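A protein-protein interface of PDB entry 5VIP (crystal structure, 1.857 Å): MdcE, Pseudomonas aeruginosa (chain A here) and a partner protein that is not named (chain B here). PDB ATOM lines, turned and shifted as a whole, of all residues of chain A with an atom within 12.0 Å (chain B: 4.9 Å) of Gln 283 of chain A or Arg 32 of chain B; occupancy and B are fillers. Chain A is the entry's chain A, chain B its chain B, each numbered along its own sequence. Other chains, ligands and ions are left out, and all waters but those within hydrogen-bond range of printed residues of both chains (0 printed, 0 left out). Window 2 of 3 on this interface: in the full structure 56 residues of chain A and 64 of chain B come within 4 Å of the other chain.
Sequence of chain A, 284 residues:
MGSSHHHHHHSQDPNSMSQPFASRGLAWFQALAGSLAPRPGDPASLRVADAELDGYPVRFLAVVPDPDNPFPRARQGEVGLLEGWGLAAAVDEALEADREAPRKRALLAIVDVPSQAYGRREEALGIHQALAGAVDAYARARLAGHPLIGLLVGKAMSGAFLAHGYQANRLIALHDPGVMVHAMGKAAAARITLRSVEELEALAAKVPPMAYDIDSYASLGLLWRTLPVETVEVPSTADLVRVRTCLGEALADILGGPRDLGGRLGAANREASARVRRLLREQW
OXT of Trp 284 of chain A lies within salt-bridge range of NE of Arg 63 of chain B, at 2.9 Å.
The guanidinium group of Arg 32 of chain B lies within hydrogen-bond range of the backbone carbonyl oxygen of Gln 283 of chain A.
The chain-end carboxylate (OXT) of Trp 284 of chain A lies within salt-bridge range of the guanidinium group (NH2) of Arg 32 of chain B (2.8 Å).
N of Leu 35 of chain B is in hydrogen-bond range of OE1 of Gln 283 of chain A (3.0 Å).
O of Val 61 of chain B lies within hydrogen-bond range of N of Leu 34 of chain B.
N of Arg 63 of chain B is in hydrogen-bond range of O of Arg 32 of chain B, 2.7 Å away.
Val 276 of chain A touches Leu 35 of chain B (CG1 to CD2, 3.9 Å).
Leu 279 of chain A touches Leu 35 of chain B.
Leu 280 of chain A touches Leu 34 of chain B (CD2 to CD1, 3.7 Å).
Leu 280 of chain A touches Leu 35 of chain B (N to CD1, 3.6 Å).
Gln 283 of chain A touches Leu 34 of chain B (O to CD2, 3.5 Å).
Leu 34 of chain B touches Trp 284 of chain A.
Ala 272 of chain A touches none of the printed residues of chain B.
Arg 275 of chain A touches none of the printed residues of chain B.
Of the printed residues of chain B, Val 276 of chain A touches Leu 35.
Printed residues of chain B within 4 Å of Leu 279 of chain A: Leu 35.
Of chain B, only Arg 32, Leu 34 and Leu 35 come within 4 Å of Gln 283 of chain A.
Printed residues of chain B within 4 Å of Trp 284 of chain A: Arg 32, Leu 34 and Arg 63.
No residue of chain A comes within 4 Å of Phe 31 of chain B.
Arg 32 of chain B touches just these residues of chain A: Gln 283 and Trp 284.
Glu 33 of chain B touches none of the printed residues of chain A.
Of chain A, only Leu 280, Gln 283 and Trp 284 come within 4 Å of Leu 34 of chain B.
Of chain A, only Val 276 (3.9 Å), Leu 279 (3.6 Å), Leu 280 (3.6 Å) and Gln 283 (3.0 Å) come within 4 Å of Leu 35 of chain B.
Arg 63 of chain B touches just one residue of chain A: Trp 284.
The nearest residue of chain B that does not touch Gln 283 of chain A is Glu 33 of chain B (4.7 Å).
Printed residues of chain B that touch a printed residue of chain A: Arg 32, Leu 34, Leu 35 and Arg 63.
Hydrophobic or aromatic side chains of chain B that line the printed part of chain A: Leu 34 and Leu 35.
Hydrophobic or aromatic side chains of chain A within 4 Å of the printed part of chain B: Val 276, Leu 279, Leu 280 and Trp 284.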
ATOM      1  N   ALA A 272     -25.324  12.226  -1.171  1.00  0.00           N
ATOM      2  CA  ALA A 272     -25.734  11.122  -2.034  1.00  0.00           C
ATOM      3  C   ALA A 272     -24.587  10.119  -2.218  1.00  0.00           C
ATOM      4  O   ALA A 272     -24.808   8.910  -2.172  1.00  0.00           O
ATOM      5  CB  ALA A 272     -26.213  11.642  -3.378  1.00  0.00           C
ATOM      6  N   SER A 273     -23.372  10.636  -2.404  1.00  0.00           N
ATOM      7  CA  SER A 273     -22.161   9.819  -2.557  1.00  0.00           C
ATOM      8  C   SER A 273     -21.880   9.017  -1.305  1.00  0.00           C
ATOM      9  O   SER A 273     -21.480   7.844  -1.364  1.00  0.00           O
ATOM     10  CB  SER A 273     -20.944  10.701  -2.859  1.00  0.00           C
ATOM     11  OG  SER A 273     -21.093  11.382  -4.084  1.00  0.00           O
ATOM     12  N   ALA A 274     -22.076   9.675  -0.167  1.00  0.00           N
ATOM     13  CA  ALA A 274     -21.831   9.064   1.122  1.00  0.00           C
ATOM     14  C   ALA A 274     -22.812   7.921   1.345  1.00  0.00           C
ATOM     15  O   ALA A 274     -22.430   6.876   1.855  1.00  0.00           O
ATOM     16  CB  ALA A 274     -21.946  10.099   2.239  1.00  0.00           C
ATOM     17  N   ARG A 275     -24.070   8.135   0.961  1.00  0.00           N
ATOM     18  CA  ARG A 275     -25.100   7.112   1.098  1.00  0.00           C
ATOM     19  C   ARG A 275     -24.773   5.894   0.241  1.00  0.00           C
ATOM     20  O   ARG A 275     -24.929   4.753   0.680  1.00  0.00           O
ATOM     21  CB  ARG A 275     -26.477   7.659   0.711  1.00  0.00           C
ATOM     22  CG  ARG A 275     -27.586   6.615   0.823  1.00  0.00           C
ATOM     23  CD  ARG A 275     -28.987   7.203   0.690  1.00  0.00           C
ATOM     24  NE  ARG A 275     -29.993   6.138   0.595  1.00  0.00           N
ATOM     25  CZ  ARG A 275     -30.585   5.563   1.639  1.00  0.00           C
ATOM     26  NH1 ARG A 275     -30.291   5.953   2.873  1.00  0.00           N
ATOM     27  NH2 ARG A 275     -31.479   4.596   1.450  1.00  0.00           N
ATOM     28  N   VAL A 276     -24.334   6.160  -0.984  1.00  0.00           N
ATOM     29  CA  VAL A 276     -23.955   5.102  -1.908  1.00  0.00           C
ATOM     30  C   VAL A 276     -22.883   4.231  -1.277  1.00  0.00           C
ATOM     31  O   VAL A 276     -23.027   3.020  -1.222  1.00  0.00           O
ATOM     32  CB  VAL A 276     -23.464   5.667  -3.254  1.00  0.00           C
ATOM     33  CG1 VAL A 276     -22.686   4.593  -4.041  1.00  0.00           C
ATOM     34  CG2 VAL A 276     -24.639   6.211  -4.064  1.00  0.00           C
ATOM     35  N   ARG A 277     -21.825   4.847  -0.764  1.00  0.00           N
ATOM     36  CA  ARG A 277     -20.725   4.084  -0.188  1.00  0.00           C
ATOM     37  C   ARG A 277     -21.147   3.322   1.065  1.00  0.00           C
ATOM     38  O   ARG A 277     -20.688   2.200   1.296  1.00  0.00           O
ATOM     39  CB  ARG A 277     -19.536   5.005   0.116  1.00  0.00           C
ATOM     40  CG  ARG A 277     -18.782   5.435  -1.140  1.00  0.00           C
ATOM     41  CD  ARG A 277     -17.513   6.211  -0.802  1.00  0.00           C
ATOM     42  NE  ARG A 277     -16.647   6.377  -1.973  1.00  0.00           N
ATOM     43  CZ  ARG A 277     -16.818   7.309  -2.908  1.00  0.00           C
ATOM     44  NH1 ARG A 277     -17.823   8.180  -2.815  1.00  0.00           N
ATOM     45  NH2 ARG A 277     -15.984   7.374  -3.938  1.00  0.00           N
ATOM     46  N   ARG A 278     -22.030   3.914   1.868  1.00  0.00           N
ATOM     47  CA  ARG A 278     -22.538   3.200   3.042  1.00  0.00           C
ATOM     48  C   ARG A 278     -23.361   1.963   2.632  1.00  0.00           C
ATOM     49  O   ARG A 278     -23.203   0.884   3.196  1.00  0.00           O
ATOM     50  CB  ARG A 278     -23.380   4.142   3.922  1.00  0.00           C
ATOM     51  CG  ARG A 278     -23.890   3.500   5.216  1.00  0.00           C
ATOM     52  CD  ARG A 278     -24.686   4.486   6.090  1.00  0.00           C
ATOM     53  NE  ARG A 278     -25.788   5.134   5.375  1.00  0.00           N
ATOM     54  CZ  ARG A 278     -26.970   4.564   5.139  1.00  0.00           C
ATOM     55  NH1 ARG A 278     -27.208   3.325   5.555  1.00  0.00           N
ATOM     56  NH2 ARG A 278     -27.915   5.230   4.484  1.00  0.00           N
ATOM     57  N   LEU A 279     -24.234   2.116   1.641  1.00  0.00           N
ATOM     58  CA  LEU A 279     -25.049   0.987   1.186  1.00  0.00           C
ATOM     59  C   LEU A 279     -24.191  -0.135   0.584  1.00  0.00           C
ATOM     60  O   LEU A 279     -24.421  -1.312   0.866  1.00  0.00           O
ATOM     61  CB  LEU A 279     -26.088   1.453   0.176  1.00  0.00           C
ATOM     62  CG  LEU A 279     -27.154   2.385   0.754  1.00  0.00           C
ATOM     63  CD1 LEU A 279     -28.069   2.915  -0.339  1.00  0.00           C
ATOM     64  CD2 LEU A 279     -27.950   1.654   1.837  1.00  0.00           C
ATOM     65  N   LEU A 280     -23.205   0.226  -0.238  1.00  0.00           N
ATOM     66  CA  LEU A 280     -22.294  -0.774  -0.802  1.00  0.00           C
ATOM     67  C   LEU A 280     -21.620  -1.603   0.279  1.00  0.00           C
ATOM     68  O   LEU A 280     -21.529  -2.818   0.164  1.00  0.00           O
ATOM     69  CB  LEU A 280     -21.217  -0.107  -1.664  1.00  0.00           C
ATOM     70  CG  LEU A 280     -21.634   0.406  -3.036  1.00  0.00           C
ATOM     71  CD1 LEU A 280     -20.507   1.215  -3.631  1.00  0.00           C
ATOM     72  CD2 LEU A 280     -21.987  -0.763  -3.936  1.00  0.00           C
ATOM     73  N   ARG A 281     -21.142  -0.944   1.329  1.00  0.00           N
ATOM     74  CA  ARG A 281     -20.468  -1.646   2.407  1.00  0.00           C
ATOM     75  C   ARG A 281     -21.405  -2.595   3.163  1.00  0.00           C
ATOM     76  O   ARG A 281     -21.016  -3.716   3.510  1.00  0.00           O
ATOM     77  CB  ARG A 281     -19.852  -0.649   3.383  1.00  0.00           C
ATOM     78  CG  ARG A 281     -18.976  -1.296   4.426  1.00  0.00           C
ATOM     79  CD  ARG A 281     -18.320  -0.238   5.311  1.00  0.00           C
ATOM     80  NE  ARG A 281     -17.291   0.528   4.608  1.00  0.00           N
ATOM     81  CZ  ARG A 281     -16.052   0.089   4.390  1.00  0.00           C
ATOM     82  NH1 ARG A 281     -15.688  -1.114   4.806  1.00  0.00           N
ATOM     83  NH2 ARG A 281     -15.175   0.851   3.749  1.00  0.00           N
ATOM     84  N   GLU A 282     -22.623  -2.127   3.425  1.00  0.00           N
ATOM     85  CA  GLU A 282     -23.655  -2.936   4.075  1.00  0.00           C
ATOM     86  C   GLU A 282     -23.994  -4.163   3.240  1.00  0.00           C
ATOM     87  O   GLU A 282     -24.218  -5.251   3.770  1.00  0.00           O
ATOM     88  CB  GLU A 282     -24.929  -2.104   4.308  1.00  0.00           C
ATOM     89  CG  GLU A 282     -24.781  -1.015   5.378  1.00  0.00           C
ATOM     90  CD  GLU A 282     -26.015  -0.140   5.533  1.00  0.00           C
ATOM     91  OE1 GLU A 282     -27.008  -0.351   4.800  1.00  0.00           O
ATOM     92  OE2 GLU A 282     -25.986   0.776   6.390  1.00  0.00           O
ATOM     93  N   GLN A 283     -24.037  -3.992   1.927  1.00  0.00           N
ATOM     94  CA  GLN A 283     -24.523  -5.066   1.065  1.00  0.00           C
ATOM     95  C   GLN A 283     -23.424  -5.929   0.431  1.00  0.00           C
ATOM     96  O   GLN A 283     -23.724  -6.936  -0.214  1.00  0.00           O
ATOM     97  CB  GLN A 283     -25.392  -4.471  -0.030  1.00  0.00           C
ATOM     98  CG  GLN A 283     -26.574  -3.692   0.507  1.00  0.00           C
ATOM     99  CD  GLN A 283     -27.381  -3.064  -0.590  1.00  0.00           C
ATOM    100  OE1 GLN A 283     -27.324  -3.506  -1.734  1.00  0.00           O
ATOM    101  NE2 GLN A 283     -28.145  -2.019  -0.253  1.00  0.00           N
ATOM    102  N   TRP A 284     -22.170  -5.534   0.619  1.00  0.00           N
ATOM    103  CA  TRP A 284     -21.018  -6.175  -0.033  1.00  0.00           C
ATOM    104  C   TRP A 284     -20.958  -7.695   0.130  1.00  0.00           C
ATOM    105  O   TRP A 284     -21.139  -8.234   1.226  1.00  0.00           O
ATOM    106  CB  TRP A 284     -19.723  -5.585   0.520  1.00  0.00           C
ATOM    107  CG  TRP A 284     -18.499  -5.905  -0.293  1.00  0.00           C
ATOM    108  CD1 TRP A 284     -17.466  -6.724   0.063  1.00  0.00           C
ATOM    109  CD2 TRP A 284     -18.173  -5.382  -1.586  1.00  0.00           C
ATOM    110  NE1 TRP A 284     -16.520  -6.749  -0.936  1.00  0.00           N
ATOM    111  CE2 TRP A 284     -16.930  -5.937  -1.959  1.00  0.00           C
ATOM    112  CE3 TRP A 284     -18.815  -4.507  -2.469  1.00  0.00           C
ATOM    113  CZ2 TRP A 284     -16.306  -5.634  -3.177  1.00  0.00           C
ATOM    114  CZ3 TRP A 284     -18.190  -4.204  -3.684  1.00  0.00           C
ATOM    115  CH2 TRP A 284     -16.952  -4.768  -4.020  1.00  0.00           C
ATOM    116  OXT TRP A 284     -20.688  -8.419  -0.832  1.00  0.00           O
ATOM    117  N   SER B  30     -24.378 -16.952  -9.120  1.00  0.00           N
ATOM    118  CA  SER B  30     -23.628 -16.060  -8.217  1.00  0.00           C
ATOM    119  C   SER B  30     -24.024 -14.578  -8.314  1.00  0.00           C
ATOM    120  O   SER B  30     -23.719 -13.792  -7.410  1.00  0.00           O
ATOM    121  CB  SER B  30     -22.116 -16.177  -8.465  1.00  0.00           C
ATOM    122  OG  SER B  30     -21.748 -15.490  -9.654  1.00  0.00           O
ATOM    123  N   PHE B  31     -24.682 -14.196  -9.407  1.00  0.00           N
ATOM    124  CA  PHE B  31     -25.042 -12.798  -9.653  1.00  0.00           C
ATOM    125  C   PHE B  31     -25.933 -12.208  -8.557  1.00  0.00           C
ATOM    126  O   PHE B  31     -27.023 -12.691  -8.285  1.00  0.00           O
ATOM    127  CB  PHE B  31     -25.740 -12.656 -11.008  1.00  0.00           C
ATOM    128  CG  PHE B  31     -26.252 -11.269 -11.290  1.00  0.00           C
ATOM    129  CD1 PHE B  31     -25.423 -10.308 -11.840  1.00  0.00           C
ATOM    130  CD2 PHE B  31     -27.565 -10.925 -11.009  1.00  0.00           C
ATOM    131  CE1 PHE B  31     -25.896  -9.026 -12.115  1.00  0.00           C
ATOM    132  CE2 PHE B  31     -28.038  -9.640 -11.266  1.00  0.00           C
ATOM    133  CZ  PHE B  31     -27.196  -8.691 -11.817  1.00  0.00           C
ATOM    134  N   ARG B  32     -25.462 -11.126  -7.967  1.00  0.00           N
ATOM    135  CA  ARG B  32     -26.118 -10.497  -6.836  1.00  0.00           C
ATOM    136  C   ARG B  32     -26.005  -8.985  -7.020  1.00  0.00           C
ATOM    137  O   ARG B  32     -24.908  -8.433  -6.857  1.00  0.00           O
ATOM    138  CB  ARG B  32     -25.427 -10.984  -5.554  1.00  0.00           C
ATOM    139  CG  ARG B  32     -26.041 -10.592  -4.266  1.00  0.00           C
ATOM    140  CD  ARG B  32     -25.537 -11.492  -3.128  1.00  0.00           C
ATOM    141  NE  ARG B  32     -24.087 -11.451  -2.884  1.00  0.00           N
ATOM    142  CZ  ARG B  32     -23.451 -10.451  -2.272  1.00  0.00           C
ATOM    143  NH1 ARG B  32     -24.121  -9.376  -1.877  1.00  0.00           N
ATOM    144  NH2 ARG B  32     -22.137 -10.518  -2.070  1.00  0.00           N
ATOM    145  N   GLU B  33     -27.092  -8.306  -7.383  1.00  0.00           N
ATOM    146  CA  GLU B  33     -26.997  -6.862  -7.627  1.00  0.00           C
ATOM    147  C   GLU B  33     -27.094  -6.001  -6.363  1.00  0.00           C
ATOM    148  O   GLU B  33     -28.008  -6.166  -5.553  1.00  0.00           O
ATOM    149  CB  GLU B  33     -28.061  -6.409  -8.632  1.00  0.00           C
ATOM    150  CG  GLU B  33     -27.917  -4.922  -8.947  1.00  0.00           C
ATOM    151  CD  GLU B  33     -28.808  -4.430 -10.075  1.00  0.00           C
ATOM    152  OE1 GLU B  33     -29.550  -5.253 -10.665  1.00  0.00           O
ATOM    153  OE2 GLU B  33     -28.740  -3.208 -10.383  1.00  0.00           O
ATOM    154  N   LEU B  34     -26.142  -5.083  -6.199  1.00  0.00           N
ATOM    155  CA  LEU B  34     -26.147  -4.166  -5.058  1.00  0.00           C
ATOM    156  C   LEU B  34     -26.874  -2.882  -5.414  1.00  0.00           C
ATOM    157  O   LEU B  34     -26.850  -2.460  -6.567  1.00  0.00           O
ATOM    158  CB  LEU B  34     -24.727  -3.824  -4.612  1.00  0.00           C
ATOM    159  CG  LEU B  34     -23.735  -4.977  -4.444  1.00  0.00           C
ATOM    160  CD1 LEU B  34     -22.438  -4.455  -3.824  1.00  0.00           C
ATOM    161  CD2 LEU B  34     -24.311  -6.108  -3.595  1.00  0.00           C
ATOM    162  N   LEU B  35     -27.490  -2.248  -4.418  1.00  0.00           N
ATOM    163  CA  LEU B  35     -28.132  -0.946  -4.627  1.00  0.00           C
ATOM    164  C   LEU B  35     -29.126  -1.039  -5.764  1.00  0.00           C
ATOM    165  O   LEU B  35     -29.208  -0.153  -6.619  1.00  0.00           O
ATOM    166  CB  LEU B  35     -27.097   0.149  -4.923  1.00  0.00           C
ATOM    167  CG  LEU B  35     -26.449   0.858  -3.733  1.00  0.00           C
ATOM    168  CD1 LEU B  35     -25.453  -0.047  -3.014  1.00  0.00           C
ATOM    169  CD2 LEU B  35     -25.786   2.157  -4.192  1.00  0.00           C
ATOM    170  N   VAL B  61     -24.121  -2.417 -10.370  1.00  0.00           N
ATOM    171  CA  VAL B  61     -23.005  -2.953  -9.604  1.00  0.00           C
ATOM    172  C   VAL B  61     -23.438  -4.305  -9.077  1.00  0.00           C
ATOM    173  O   VAL B  61     -24.478  -4.420  -8.409  1.00  0.00           O
ATOM    174  CB  VAL B  61     -22.580  -2.039  -8.446  1.00  0.00           C
ATOM    175  CG1 VAL B  61     -21.639  -2.789  -7.510  1.00  0.00           C
ATOM    176  CG2 VAL B  61     -21.915  -0.781  -8.998  1.00  0.00           C
ATOM    177  N   ALA B  62     -22.663  -5.335  -9.397  1.00  0.00           N
ATOM    178  CA  ALA B  62     -23.053  -6.687  -9.013  1.00  0.00           C
ATOM    179  C   ALA B  62     -21.902  -7.436  -8.388  1.00  0.00           C
ATOM    180  O   ALA B  62     -20.755  -7.278  -8.795  1.00  0.00           O
ATOM    181  CB  ALA B  62     -23.577  -7.445 -10.218  1.00  0.00           C
ATOM    182  N   ARG B  63     -22.220  -8.253  -7.392  1.00  0.00           N
ATOM    183  CA  ARG B  63     -21.252  -9.147  -6.784  1.00  0.00           C
ATOM    184  C   ARG B  63     -21.475 -10.542  -7.350  1.00  0.00           C
ATOM    185  O   ARG B  63     -22.574 -10.878  -7.806  1.00  0.00           O
ATOM    186  CB  ARG B  63     -21.386  -9.126  -5.263  1.00  0.00           C
ATOM    187  CG  ARG B  63     -20.859  -7.839  -4.619  1.00  0.00           C
ATOM    188  CD  ARG B  63     -19.332  -7.899  -4.487  1.00  0.00           C
ATOM    189  NE  ARG B  63     -18.981  -8.463  -3.188  1.00  0.00           N
ATOM    190  CZ  ARG B  63     -18.046  -9.371  -2.973  1.00  0.00           C
ATOM    191  NH1 ARG B  63     -17.312  -9.850  -3.978  1.00  0.00           N
ATOM    192  NH2 ARG B  63     -17.846  -9.804  -1.736  1.00  0.00           N
